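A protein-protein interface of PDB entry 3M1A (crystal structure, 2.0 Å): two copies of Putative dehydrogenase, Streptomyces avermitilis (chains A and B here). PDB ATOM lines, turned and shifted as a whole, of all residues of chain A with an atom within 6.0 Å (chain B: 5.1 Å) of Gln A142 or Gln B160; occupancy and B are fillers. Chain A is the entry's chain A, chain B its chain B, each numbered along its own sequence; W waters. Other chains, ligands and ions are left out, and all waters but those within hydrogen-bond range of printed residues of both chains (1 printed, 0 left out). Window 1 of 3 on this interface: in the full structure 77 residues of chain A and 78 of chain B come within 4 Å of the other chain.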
ATOM      1  N   SER A 137     -23.689   9.238 -14.532  1.00  0.00           N
ATOM      2  CA  SER A 137     -24.257   9.818 -15.714  1.00  0.00           C
ATOM      3  C   SER A 137     -25.498   9.021 -16.157  1.00  0.00           C
ATOM      4  O   SER A 137     -26.361   8.652 -15.328  1.00  0.00           O
ATOM      5  CB  SER A 137     -23.185   9.845 -16.821  1.00  0.00           C
ATOM      6  OG  SER A 137     -23.650  10.491 -17.989  1.00  0.00           O
ATOM      7  N   SER A 138     -25.588   8.751 -17.455  1.00  0.00           N
ATOM      8  CA  SER A 138     -26.780   8.106 -18.054  1.00  0.00           C
ATOM      9  C   SER A 138     -26.426   7.777 -19.502  1.00  0.00           C
ATOM     10  O   SER A 138     -25.415   8.263 -19.996  1.00  0.00           O
ATOM     11  CB  SER A 138     -27.951   9.108 -18.009  1.00  0.00           C
ATOM     12  OG  SER A 138     -28.983   8.804 -18.946  1.00  0.00           O
ATOM     13  N   PHE A 139     -27.214   6.966 -20.209  1.00  0.00           N
ATOM     14  CA  PHE A 139     -27.045   6.894 -21.662  1.00  0.00           C
ATOM     15  C   PHE A 139     -27.190   8.325 -22.228  1.00  0.00           C
ATOM     16  O   PHE A 139     -26.548   8.675 -23.219  1.00  0.00           O
ATOM     17  CB  PHE A 139     -28.011   5.882 -22.318  1.00  0.00           C
ATOM     18  CG  PHE A 139     -29.484   6.124 -21.974  1.00  0.00           C
ATOM     19  CD1 PHE A 139     -30.257   7.024 -22.711  1.00  0.00           C
ATOM     20  CD2 PHE A 139     -30.074   5.475 -20.882  1.00  0.00           C
ATOM     21  CE1 PHE A 139     -31.607   7.261 -22.380  1.00  0.00           C
ATOM     22  CE2 PHE A 139     -31.406   5.710 -20.532  1.00  0.00           C
ATOM     23  CZ  PHE A 139     -32.181   6.599 -21.280  1.00  0.00           C
ATOM     24  N   GLY A 140     -27.941   9.181 -21.523  1.00  0.00           N
ATOM     25  CA  GLY A 140     -28.187  10.560 -21.944  1.00  0.00           C
ATOM     26  C   GLY A 140     -26.964  11.453 -21.868  1.00  0.00           C
ATOM     27  O   GLY A 140     -26.992  12.575 -22.334  1.00  0.00           O
ATOM     28  N   GLY A 141     -25.869  10.953 -21.293  1.00  0.00           N
ATOM     29  CA  GLY A 141     -24.605  11.698 -21.331  1.00  0.00           C
ATOM     30  C   GLY A 141     -23.951  11.730 -22.705  1.00  0.00           C
ATOM     31  O   GLY A 141     -23.013  12.509 -22.907  1.00  0.00           O
ATOM     32  N   GLN A 142     -24.427  10.875 -23.630  1.00  0.00           N
ATOM     33  CA  GLN A 142     -23.888  10.809 -24.998  1.00  0.00           C
ATOM     34  C   GLN A 142     -24.927  11.173 -26.079  1.00  0.00           C
ATOM     35  O   GLN A 142     -24.591  11.297 -27.264  1.00  0.00           O
ATOM     36  CB  GLN A 142     -23.344   9.393 -25.300  1.00  0.00           C
ATOM     37  CG  GLN A 142     -22.021   9.004 -24.611  1.00  0.00           C
ATOM     38  CD  GLN A 142     -21.536   7.611 -25.037  1.00  0.00           C
ATOM     39  OE1 GLN A 142     -21.167   6.796 -24.204  1.00  0.00           O
ATOM     40  NE2 GLN A 142     -21.551   7.338 -26.345  1.00  0.00           N
ATOM     41  N   LEU A 143     -26.189  11.322 -25.695  1.00  0.00           N
ATOM     42  CA  LEU A 143     -27.262  11.471 -26.678  1.00  0.00           C
ATOM     43  C   LEU A 143     -28.514  12.102 -26.082  1.00  0.00           C
ATOM     44  O   LEU A 143     -28.712  12.080 -24.867  1.00  0.00           O
ATOM     45  CB  LEU A 143     -27.632  10.099 -27.244  1.00  0.00           C
ATOM     46  CG  LEU A 143     -28.289   9.114 -26.260  1.00  0.00           C
ATOM     47  CD1 LEU A 143     -29.796   8.952 -26.509  1.00  0.00           C
ATOM     48  CD2 LEU A 143     -27.621   7.758 -26.359  1.00  0.00           C
ATOM     49  N   SER A 144     -29.369  12.656 -26.938  1.00  0.00           N
ATOM     50  CA  SER A 144     -30.622  13.221 -26.456  1.00  0.00           C
ATOM     51  C   SER A 144     -31.720  12.999 -27.470  1.00  0.00           C
ATOM     52  O   SER A 144     -31.464  12.488 -28.571  1.00  0.00           O
ATOM     53  CB  SER A 144     -30.492  14.711 -26.156  1.00  0.00           C
ATOM     54  OG  SER A 144     -31.569  15.086 -25.339  1.00  0.00           O
ATOM     55  N   PHE A 145     -32.934  13.391 -27.081  1.00  0.00           N
ATOM     56  CA  PHE A 145     -34.131  13.280 -27.890  1.00  0.00           C
ATOM     57  C   PHE A 145     -35.195  14.145 -27.227  1.00  0.00           C
ATOM     58  O   PHE A 145     -34.928  14.805 -26.229  1.00  0.00           O
ATOM     59  CB  PHE A 145     -34.586  11.800 -28.034  1.00  0.00           C
ATOM     60  CG  PHE A 145     -34.461  10.980 -26.761  1.00  0.00           C
ATOM     61  CD1 PHE A 145     -33.380  10.099 -26.584  1.00  0.00           C
ATOM     62  CD2 PHE A 145     -35.443  11.051 -25.761  1.00  0.00           C
ATOM     63  CE1 PHE A 145     -33.267   9.323 -25.410  1.00  0.00           C
ATOM     64  CE2 PHE A 145     -35.348  10.272 -24.593  1.00  0.00           C
ATOM     65  CZ  PHE A 145     -34.259   9.417 -24.413  1.00  0.00           C
ATOM     66  N   PHE A 148     -35.665  15.599 -23.401  1.00  0.00           N
ATOM     67  CA  PHE A 148     -34.493  15.215 -22.608  1.00  0.00           C
ATOM     68  C   PHE A 148     -33.341  16.192 -22.773  1.00  0.00           C
ATOM     69  O   PHE A 148     -32.225  15.901 -22.357  1.00  0.00           O
ATOM     70  CB  PHE A 148     -34.008  13.851 -23.057  1.00  0.00           C
ATOM     71  CG  PHE A 148     -33.840  12.834 -21.943  1.00  0.00           C
ATOM     72  CD1 PHE A 148     -32.752  11.952 -21.957  1.00  0.00           C
ATOM     73  CD2 PHE A 148     -34.780  12.720 -20.924  1.00  0.00           C
ATOM     74  CE1 PHE A 148     -32.581  10.972 -20.965  1.00  0.00           C
ATOM     75  CE2 PHE A 148     -34.626  11.732 -19.907  1.00  0.00           C
ATOM     76  CZ  PHE A 148     -33.528  10.856 -19.935  1.00  0.00           C
ATOM     77  N   SER A 149     -33.604  17.343 -23.386  1.00  0.00           N
ATOM     78  CA  SER A 149     -32.524  18.257 -23.733  1.00  0.00           C
ATOM     79  C   SER A 149     -31.728  18.758 -22.533  1.00  0.00           C
ATOM     80  O   SER A 149     -30.490  18.702 -22.561  1.00  0.00           O
ATOM     81  CB  SER A 149     -33.005  19.400 -24.654  1.00  0.00           C
ATOM     82  OG  SER A 149     -33.787  20.314 -23.933  1.00  0.00           O
ATOM     83  N   SER A 152     -29.837  15.617 -20.792  1.00  0.00           N
ATOM     84  CA  SER A 152     -28.699  15.203 -21.587  1.00  0.00           C
ATOM     85  C   SER A 152     -27.576  16.278 -21.544  1.00  0.00           C
ATOM     86  O   SER A 152     -26.417  15.978 -21.374  1.00  0.00           O
ATOM     87  CB  SER A 152     -29.166  14.928 -23.013  1.00  0.00           C
ATOM     88  OG  SER A 152     -30.054  13.797 -23.041  1.00  0.00           O
ATOM     89  N   ALA A 153     -27.951  17.541 -21.691  1.00  0.00           N
ATOM     90  CA  ALA A 153     -26.968  18.604 -21.641  1.00  0.00           C
ATOM     91  C   ALA A 153     -26.125  18.578 -20.364  1.00  0.00           C
ATOM     92  O   ALA A 153     -24.900  18.702 -20.448  1.00  0.00           O
ATOM     93  CB  ALA A 153     -27.622  19.971 -21.900  1.00  0.00           C
ATOM     94  N   THR A 154     -26.756  18.387 -19.196  1.00  0.00           N
ATOM     95  CA  THR A 154     -26.009  18.342 -17.920  1.00  0.00           C
ATOM     96  C   THR A 154     -25.163  17.072 -17.817  1.00  0.00           C
ATOM     97  O   THR A 154     -24.042  17.136 -17.362  1.00  0.00           O
ATOM     98  CB  THR A 154     -26.907  18.478 -16.650  1.00  0.00           C
ATOM     99  OG1 THR A 154     -27.768  17.329 -16.530  1.00  0.00           O
ATOM    100  CG2 THR A 154     -27.732  19.776 -16.664  1.00  0.00           C
ATOM    101  N   LYS A 155     -25.686  15.931 -18.253  1.00  0.00           N
ATOM    102  CA  LYS A 155     -24.934  14.677 -18.159  1.00  0.00           C
ATOM    103  C   LYS A 155     -23.725  14.661 -19.132  1.00  0.00           C
ATOM    104  O   LYS A 155     -22.638  14.207 -18.774  1.00  0.00           O
ATOM    105  CB  LYS A 155     -25.846  13.450 -18.349  1.00  0.00           C
ATOM    106  CG  LYS A 155     -26.849  13.170 -17.208  1.00  0.00           C
ATOM    107  CD  LYS A 155     -26.196  13.297 -15.798  1.00  0.00           C
ATOM    108  CE  LYS A 155     -27.145  12.887 -14.646  1.00  0.00           C
ATOM    109  NZ  LYS A 155     -26.330  12.666 -13.410  1.00  0.00           N
ATOM    110  N   ALA A 156     -23.904  15.207 -20.330  1.00  0.00           N
ATOM    111  CA  ALA A 156     -22.827  15.264 -21.282  1.00  0.00           C
ATOM    112  C   ALA A 156     -21.721  16.200 -20.758  1.00  0.00           C
ATOM    113  O   ALA A 156     -20.537  15.927 -20.950  1.00  0.00           O
ATOM    114  CB  ALA A 156     -23.330  15.736 -22.666  1.00  0.00           C
ATOM    115  N   GLU A 159     -19.839  14.255 -18.301  1.00  0.00           N
ATOM    116  CA  GLU A 159     -19.000  13.285 -19.029  1.00  0.00           C
ATOM    117  C   GLU A 159     -17.710  13.878 -19.582  1.00  0.00           C
ATOM    118  O   GLU A 159     -16.639  13.253 -19.487  1.00  0.00           O
ATOM    119  CB  GLU A 159     -19.775  12.580 -20.157  1.00  0.00           C
ATOM    120  CG  GLU A 159     -20.856  11.688 -19.639  1.00  0.00           C
ATOM    121  CD  GLU A 159     -21.096  10.418 -20.476  1.00  0.00           C
ATOM    122  OE1 GLU A 159     -20.402  10.133 -21.485  1.00  0.00           O
ATOM    123  OE2 GLU A 159     -22.014   9.688 -20.108  1.00  0.00           O
ATOM    124  N   GLU A 180     -23.137   4.853 -16.825  1.00  0.00           N
ATOM    125  CA  GLU A 180     -24.225   5.243 -17.753  1.00  0.00           C
ATOM    126  C   GLU A 180     -25.396   4.253 -17.649  1.00  0.00           C
ATOM    127  O   GLU A 180     -25.543   3.355 -18.490  1.00  0.00           O
ATOM    128  CB  GLU A 180     -23.700   5.300 -19.187  1.00  0.00           C
ATOM    129  CG  GLU A 180     -22.649   6.357 -19.405  1.00  0.00           C
ATOM    130  CD  GLU A 180     -21.974   6.309 -20.782  1.00  0.00           C
ATOM    131  OE1 GLU A 180     -21.670   5.216 -21.256  1.00  0.00           O
ATOM    132  OE2 GLU A 180     -21.726   7.388 -21.381  1.00  0.00           O
ATOM    133  N   ARG A 244     -15.949   4.412 -19.290  1.00  0.00           N
ATOM    134  CA  ARG A 244     -17.410   4.387 -19.252  1.00  0.00           C
ATOM    135  C   ARG A 244     -17.924   2.987 -18.931  1.00  0.00           C
ATOM    136  O   ARG A 244     -17.419   2.011 -19.446  1.00  0.00           O
ATOM    137  CB  ARG A 244     -17.990   4.784 -20.612  1.00  0.00           C
ATOM    138  CG  ARG A 244     -18.074   6.259 -20.820  1.00  0.00           C
ATOM    139  CD  ARG A 244     -18.617   6.601 -22.240  1.00  0.00           C
ATOM    140  NE  ARG A 244     -18.617   8.063 -22.352  1.00  0.00           N
ATOM    141  CZ  ARG A 244     -17.558   8.792 -22.696  1.00  0.00           C
ATOM    142  NH1 ARG A 244     -16.407   8.208 -23.033  1.00  0.00           N
ATOM    143  NH2 ARG A 244     -17.652  10.123 -22.718  1.00  0.00           N
ATOM    144  N   LEU A 255     -27.006   3.604 -26.634  1.00  0.00           N
ATOM    145  CA  LEU A 255     -25.646   4.040 -26.941  1.00  0.00           C
ATOM    146  C   LEU A 255     -25.168   3.572 -28.295  1.00  0.00           C
ATOM    147  O   LEU A 255     -24.560   4.364 -29.020  1.00  0.00           O
ATOM    148  CB  LEU A 255     -24.656   3.684 -25.827  1.00  0.00           C
ATOM    149  CG  LEU A 255     -24.939   4.351 -24.472  1.00  0.00           C
ATOM    150  CD1 LEU A 255     -24.174   3.631 -23.367  1.00  0.00           C
ATOM    151  CD2 LEU A 255     -24.585   5.870 -24.510  1.00  0.00           C
ATOM    152  N   HIS A 258     -26.962   5.532 -31.178  1.00  0.00           N
ATOM    153  CA  HIS A 258     -26.333   6.840 -31.354  1.00  0.00           C
ATOM    154  C   HIS A 258     -24.933   6.787 -31.995  1.00  0.00           C
ATOM    155  O   HIS A 258     -24.630   7.592 -32.879  1.00  0.00           O
ATOM    156  CB  HIS A 258     -26.273   7.548 -30.016  1.00  0.00           C
ATOM    157  CG  HIS A 258     -25.853   8.983 -30.112  1.00  0.00           C
ATOM    158  ND1 HIS A 258     -24.568   9.386 -29.819  1.00  0.00           N
ATOM    159  CD2 HIS A 258     -26.543  10.103 -30.457  1.00  0.00           C
ATOM    160  CE1 HIS A 258     -24.481  10.695 -29.979  1.00  0.00           C
ATOM    161  NE2 HIS A 258     -25.664  11.154 -30.368  1.00  0.00           N
ATOM    162  N   LEU A 259     -24.078   5.867 -31.546  1.00  0.00           N
ATOM    163  CA  LEU A 259     -22.795   5.606 -32.244  1.00  0.00           C
ATOM    164  C   LEU A 259     -22.974   5.347 -33.733  1.00  0.00           C
ATOM    165  O   LEU A 259     -22.287   5.943 -34.572  1.00  0.00           O
ATOM    166  CB  LEU A 259     -22.024   4.427 -31.600  1.00  0.00           C
ATOM    167  CG  LEU A 259     -21.413   4.647 -30.204  1.00  0.00           C
ATOM    168  CD1 LEU A 259     -20.848   3.333 -29.602  1.00  0.00           C
ATOM    169  CD2 LEU A 259     -20.345   5.730 -30.233  1.00  0.00           C
ATOM    170  N   ALA B 156     -20.249  20.149 -25.292  1.00  0.00           N
ATOM    171  CA  ALA B 156     -21.062  18.926 -25.208  1.00  0.00           C
ATOM    172  C   ALA B 156     -22.475  19.230 -24.695  1.00  0.00           C
ATOM    173  O   ALA B 156     -23.462  18.720 -25.221  1.00  0.00           O
ATOM    174  CB  ALA B 156     -20.370  17.910 -24.302  1.00  0.00           C
ATOM    175  N   ALA B 157     -22.553  20.061 -23.652  1.00  0.00           N
ATOM    176  CA  ALA B 157     -23.820  20.620 -23.176  1.00  0.00           C
ATOM    177  C   ALA B 157     -24.629  21.267 -24.306  1.00  0.00           C
ATOM    178  O   ALA B 157     -25.805  20.942 -24.500  1.00  0.00           O
ATOM    179  CB  ALA B 157     -23.590  21.617 -22.033  1.00  0.00           C
ATOM    180  N   LEU B 158     -24.003  22.172 -25.050  1.00  0.00           N
ATOM    181  CA  LEU B 158     -24.608  22.732 -26.271  1.00  0.00           C
ATOM    182  C   LEU B 158     -25.037  21.689 -27.302  1.00  0.00           C
ATOM    183  O   LEU B 158     -26.144  21.777 -27.832  1.00  0.00           O
ATOM    184  CB  LEU B 158     -23.663  23.741 -26.933  1.00  0.00           C
ATOM    185  CG  LEU B 158     -24.123  24.468 -28.202  1.00  0.00           C
ATOM    186  CD1 LEU B 158     -25.277  25.419 -27.897  1.00  0.00           C
ATOM    187  CD2 LEU B 158     -22.943  25.203 -28.879  1.00  0.00           C
ATOM    188  N   GLU B 159     -24.183  20.696 -27.566  1.00  0.00           N
ATOM    189  CA  GLU B 159     -24.546  19.638 -28.520  1.00  0.00           C
ATOM    190  C   GLU B 159     -25.802  18.904 -28.112  1.00  0.00           C
ATOM    191  O   GLU B 159     -26.647  18.657 -28.939  1.00  0.00           O
ATOM    192  CB  GLU B 159     -23.406  18.626 -28.745  1.00  0.00           C
ATOM    193  CG  GLU B 159     -22.250  19.283 -29.480  1.00  0.00           C
ATOM    194  CD  GLU B 159     -21.526  18.377 -30.409  1.00  0.00           C
ATOM    195  OE1 GLU B 159     -21.968  17.223 -30.601  1.00  0.00           O
ATOM    196  OE2 GLU B 159     -20.505  18.836 -30.978  1.00  0.00           O
ATOM    197  N   GLN B 160     -25.899  18.549 -26.847  1.00  0.00           N
ATOM    198  CA  GLN B 160     -27.033  17.791 -26.343  1.00  0.00           C
ATOM    199  C   GLN B 160     -28.329  18.578 -26.262  1.00  0.00           C
ATOM    200  O   GLN B 160     -29.382  18.042 -26.566  1.00  0.00           O
ATOM    201  CB  GLN B 160     -26.700  17.082 -25.027  1.00  0.00           C
ATOM    202  CG  GLN B 160     -25.605  16.048 -25.189  1.00  0.00           C
ATOM    203  CD  GLN B 160     -25.849  15.076 -26.335  1.00  0.00           C
ATOM    204  OE1 GLN B 160     -26.979  14.665 -26.584  1.00  0.00           O
ATOM    205  NE2 GLN B 160     -24.771  14.698 -27.040  1.00  0.00           N
ATOM    206  N   LEU B 161     -28.250  19.852 -25.897  1.00  0.00           N
ATOM    207  CA  LEU B 161     -29.371  20.754 -26.059  1.00  0.00           C
ATOM    208  C   LEU B 161     -29.840  20.805 -27.505  1.00  0.00           C
ATOM    209  O   LEU B 161     -31.052  20.833 -27.795  1.00  0.00           O
ATOM    210  CB  LEU B 161     -28.946  22.154 -25.620  1.00  0.00           C
ATOM    211  CG  LEU B 161     -29.469  22.871 -24.377  1.00  0.00           C
ATOM    212  CD1 LEU B 161     -30.191  22.058 -23.305  1.00  0.00           C
ATOM    213  CD2 LEU B 161     -28.380  23.741 -23.800  1.00  0.00           C
ATOM    214  N   SER B 162     -28.881  20.871 -28.427  1.00  0.00           N
ATOM    215  CA  SER B 162     -29.212  20.819 -29.833  1.00  0.00           C
ATOM    216  C   SER B 162     -29.862  19.500 -30.246  1.00  0.00           C
ATOM    217  O   SER B 162     -30.836  19.534 -30.989  1.00  0.00           O
ATOM    218  CB  SER B 162     -27.993  21.112 -30.702  1.00  0.00           C
ATOM    219  OG  SER B 162     -27.426  22.347 -30.346  1.00  0.00           O
ATOM    220  N   GLU B 163     -29.328  18.346 -29.810  1.00  0.00           N
ATOM    221  CA  GLU B 163     -29.930  17.060 -30.189  1.00  0.00           C
ATOM    222  C   GLU B 163     -31.400  16.991 -29.787  1.00  0.00           C
ATOM    223  O   GLU B 163     -32.258  16.638 -30.598  1.00  0.00           O
ATOM    224  CB  GLU B 163     -29.230  15.842 -29.551  1.00  0.00           C
ATOM    225  CG  GLU B 163     -27.881  15.519 -30.092  1.00  0.00           C
ATOM    226  CD  GLU B 163     -27.500  14.020 -30.060  1.00  0.00           C
ATOM    227  OE1 GLU B 163     -28.277  13.080 -29.719  1.00  0.00           O
ATOM    228  OE2 GLU B 163     -26.354  13.794 -30.417  1.00  0.00           O
ATOM    229  N   GLY B 164     -31.672  17.217 -28.507  1.00  0.00           N
ATOM    230  CA  GLY B 164     -33.041  17.187 -27.989  1.00  0.00           C
ATOM    231  C   GLY B 164     -33.955  18.177 -28.692  1.00  0.00           C
ATOM    232  O   GLY B 164     -35.055  17.814 -29.128  1.00  0.00           O
ATOM    233  N   LEU B 165     -33.493  19.414 -28.856  1.00  0.00           N
ATOM    234  CA  LEU B 165     -34.234  20.414 -29.645  1.00  0.00           C
ATOM    235  C   LEU B 165     -34.563  19.952 -31.080  1.00  0.00           C
ATOM    236  O   LEU B 165     -35.737  20.046 -31.525  1.00  0.00           O
ATOM    237  CB  LEU B 165     -33.480  21.742 -29.672  1.00  0.00           C
ATOM    238  CG  LEU B 165     -34.055  22.858 -30.540  1.00  0.00           C
ATOM    239  CD1 LEU B 165     -35.303  23.533 -29.921  1.00  0.00           C
ATOM    240  CD2 LEU B 165     -32.980  23.889 -30.823  1.00  0.00           C
ATOM    241  N   ARG B 244     -25.158  17.106 -37.510  1.00  0.00           N
ATOM    242  CA  ARG B 244     -23.782  17.531 -37.266  1.00  0.00           C
ATOM    243  C   ARG B 244     -23.032  17.716 -38.569  1.00  0.00           C
ATOM    244  O   ARG B 244     -23.140  16.895 -39.464  1.00  0.00           O
ATOM    245  CB  ARG B 244     -23.023  16.515 -36.398  1.00  0.00           C
ATOM    246  CG  ARG B 244     -23.466  16.496 -34.944  1.00  0.00           C
ATOM    247  CD  ARG B 244     -22.733  15.389 -34.152  1.00  0.00           C
ATOM    248  NE  ARG B 244     -23.065  15.520 -32.740  1.00  0.00           N
ATOM    249  CZ  ARG B 244     -24.139  15.000 -32.157  1.00  0.00           C
ATOM    250  NH1 ARG B 244     -24.970  14.225 -32.858  1.00  0.00           N
ATOM    251  NH2 ARG B 244     -24.371  15.246 -30.856  1.00  0.00           N
ATOM    252  N   VAL B 262     -14.975   4.516 -27.868  1.00  0.00           N
ATOM    253  CA  VAL B 262     -16.231   4.401 -27.111  1.00  0.00           C
ATOM    254  C   VAL B 262     -16.935   3.094 -27.469  1.00  0.00           C
ATOM    255  O   VAL B 262     -17.376   2.355 -26.578  1.00  0.00           O
ATOM    256  CB  VAL B 262     -17.168   5.601 -27.324  1.00  0.00           C
ATOM    257  CG1 VAL B 262     -18.575   5.256 -26.818  1.00  0.00           C
ATOM    258  CG2 VAL B 262     -16.619   6.853 -26.591  1.00  0.00           C
HETATM  259  O   HOH W   1     -27.299  12.265 -33.066  1.00  0.00           O
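Gln A142 touches Val B262 (NE2 to CG1, 3.7 Å). CB of Ser A144 touches N of Gly B164, 3.6 Å away. Phe A145 touches Gly B164. Ser A149 touches Leu B161 (O to CD1, 3.5 Å). Ala A153 touches Ala B157. Ala A153 touches Gln B160. Leu B161 touches Ala A153 (CD1 to CB, 3.6 Å). Ala A156 touches Gln B160 (CB to CG, 3.4 Å). NH1 of Arg A244 touches CG2 of Val B262, at 3.8 Å. Val B262 touches Leu A259.
Printed residues of chain A that touch a printed residue of chain B: Gln A142, Leu A143, Ser A144, Phe A145, Ser A149, Ser A152, Ala A153, Ala A156, Arg A244, His A258 and Leu A259. Hydrophobic or aromatic side chains of chain A that line the printed part of chain B: Leu A143, Ala A153, Ala A156, His A258 and Leu A259. Of the 12 printed residues of chain B, 7 touch a printed residue of chain A. Printed residues of chain B that touch a printed residue of chain A: Ala B156, Ala B157, Gln B160, Leu B161, Glu B163, Gly B164 and Val B262. Among the printed residues, 18 pairs touch across the chains.
The backbone carbonyl oxygen (O) of Phe A148 sits at hydrogen-bond distance from the side-chain hydroxyl (OG) of Ser A144, at 3.2 Å. The backbone carbonyl oxygen of Gly A140 lies close to the side-chain hydroxyl of Ser A152, at 3.4 Å. NH2 of Arg B244 lies within salt-bridge range of OE2 of Glu B163 (2.5 Å). The side-chain carboxylate of Glu A159 is in salt-bridge range of the guanidinium group of Arg A244 (2.9 Å). OG of Ser A152 lies within hydrogen-bond range of O of Leu A143 (2.8 Å). OE2 of Glu A180 lies close to OE1 of Gln A142 (2.9 Å).
O of Gln A142 is in hydrogen-bond range of NE2 of Gln B160 (3.4 Å). A ring nitrogen (NE2) of His A258 lies within hydrogen-bond range of the side-chain carboxylate of Glu B163, at 2.7 Å. The backbone NH (N) of Ser A144 lies within hydrogen-bond range of the side-chain carboxylate (OE1) of Glu B163, at 3.0 Å. The backbone NH (N) of Ser A144 lies within hydrogen-bond range of the side-chain amide oxygen (OE1) of Gln B160.
Water W1 lies within hydrogen-bond range of the guanidinium group of Arg B244, the side-chain carboxylate of Glu B163 and a ring nitrogen (NE2) of His A258.
Printed residues of chain B within 4 Å of Gln A142: Gln B160 (3.4 Å) and Val B262 (3.7 Å). Printed residues of chain B within 4 Å of Leu A143: Gln B160 and Glu B163. Of the printed residues of chain B, Leu A259 touches Val B262 (3.9 Å). Printed residues of chain B within 4 Å of Arg A244: Val B262 (3.8 Å). Of the printed residues of chain A, Gly B164 touches Ser A144 and Phe A145. Of the printed residues of chain B, Ser A144 touches Gln B160 (3.1 Å), Glu B163 (3.0 Å) and Gly B164 (3.6 Å). The nearest printed residue of chain B that does not touch Gln A142 is Glu B163 (4.4 Å). The nearest printed residue of chain A that does not touch Gln B160 is Ser A149 (4.2 Å). The nearest printed residue of chain A that does not touch Glu B163 is Gln A142 (4.4 Å).
Ala A156 touches its own counterpart, Ala B156. 3 positions are printed for both chains.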
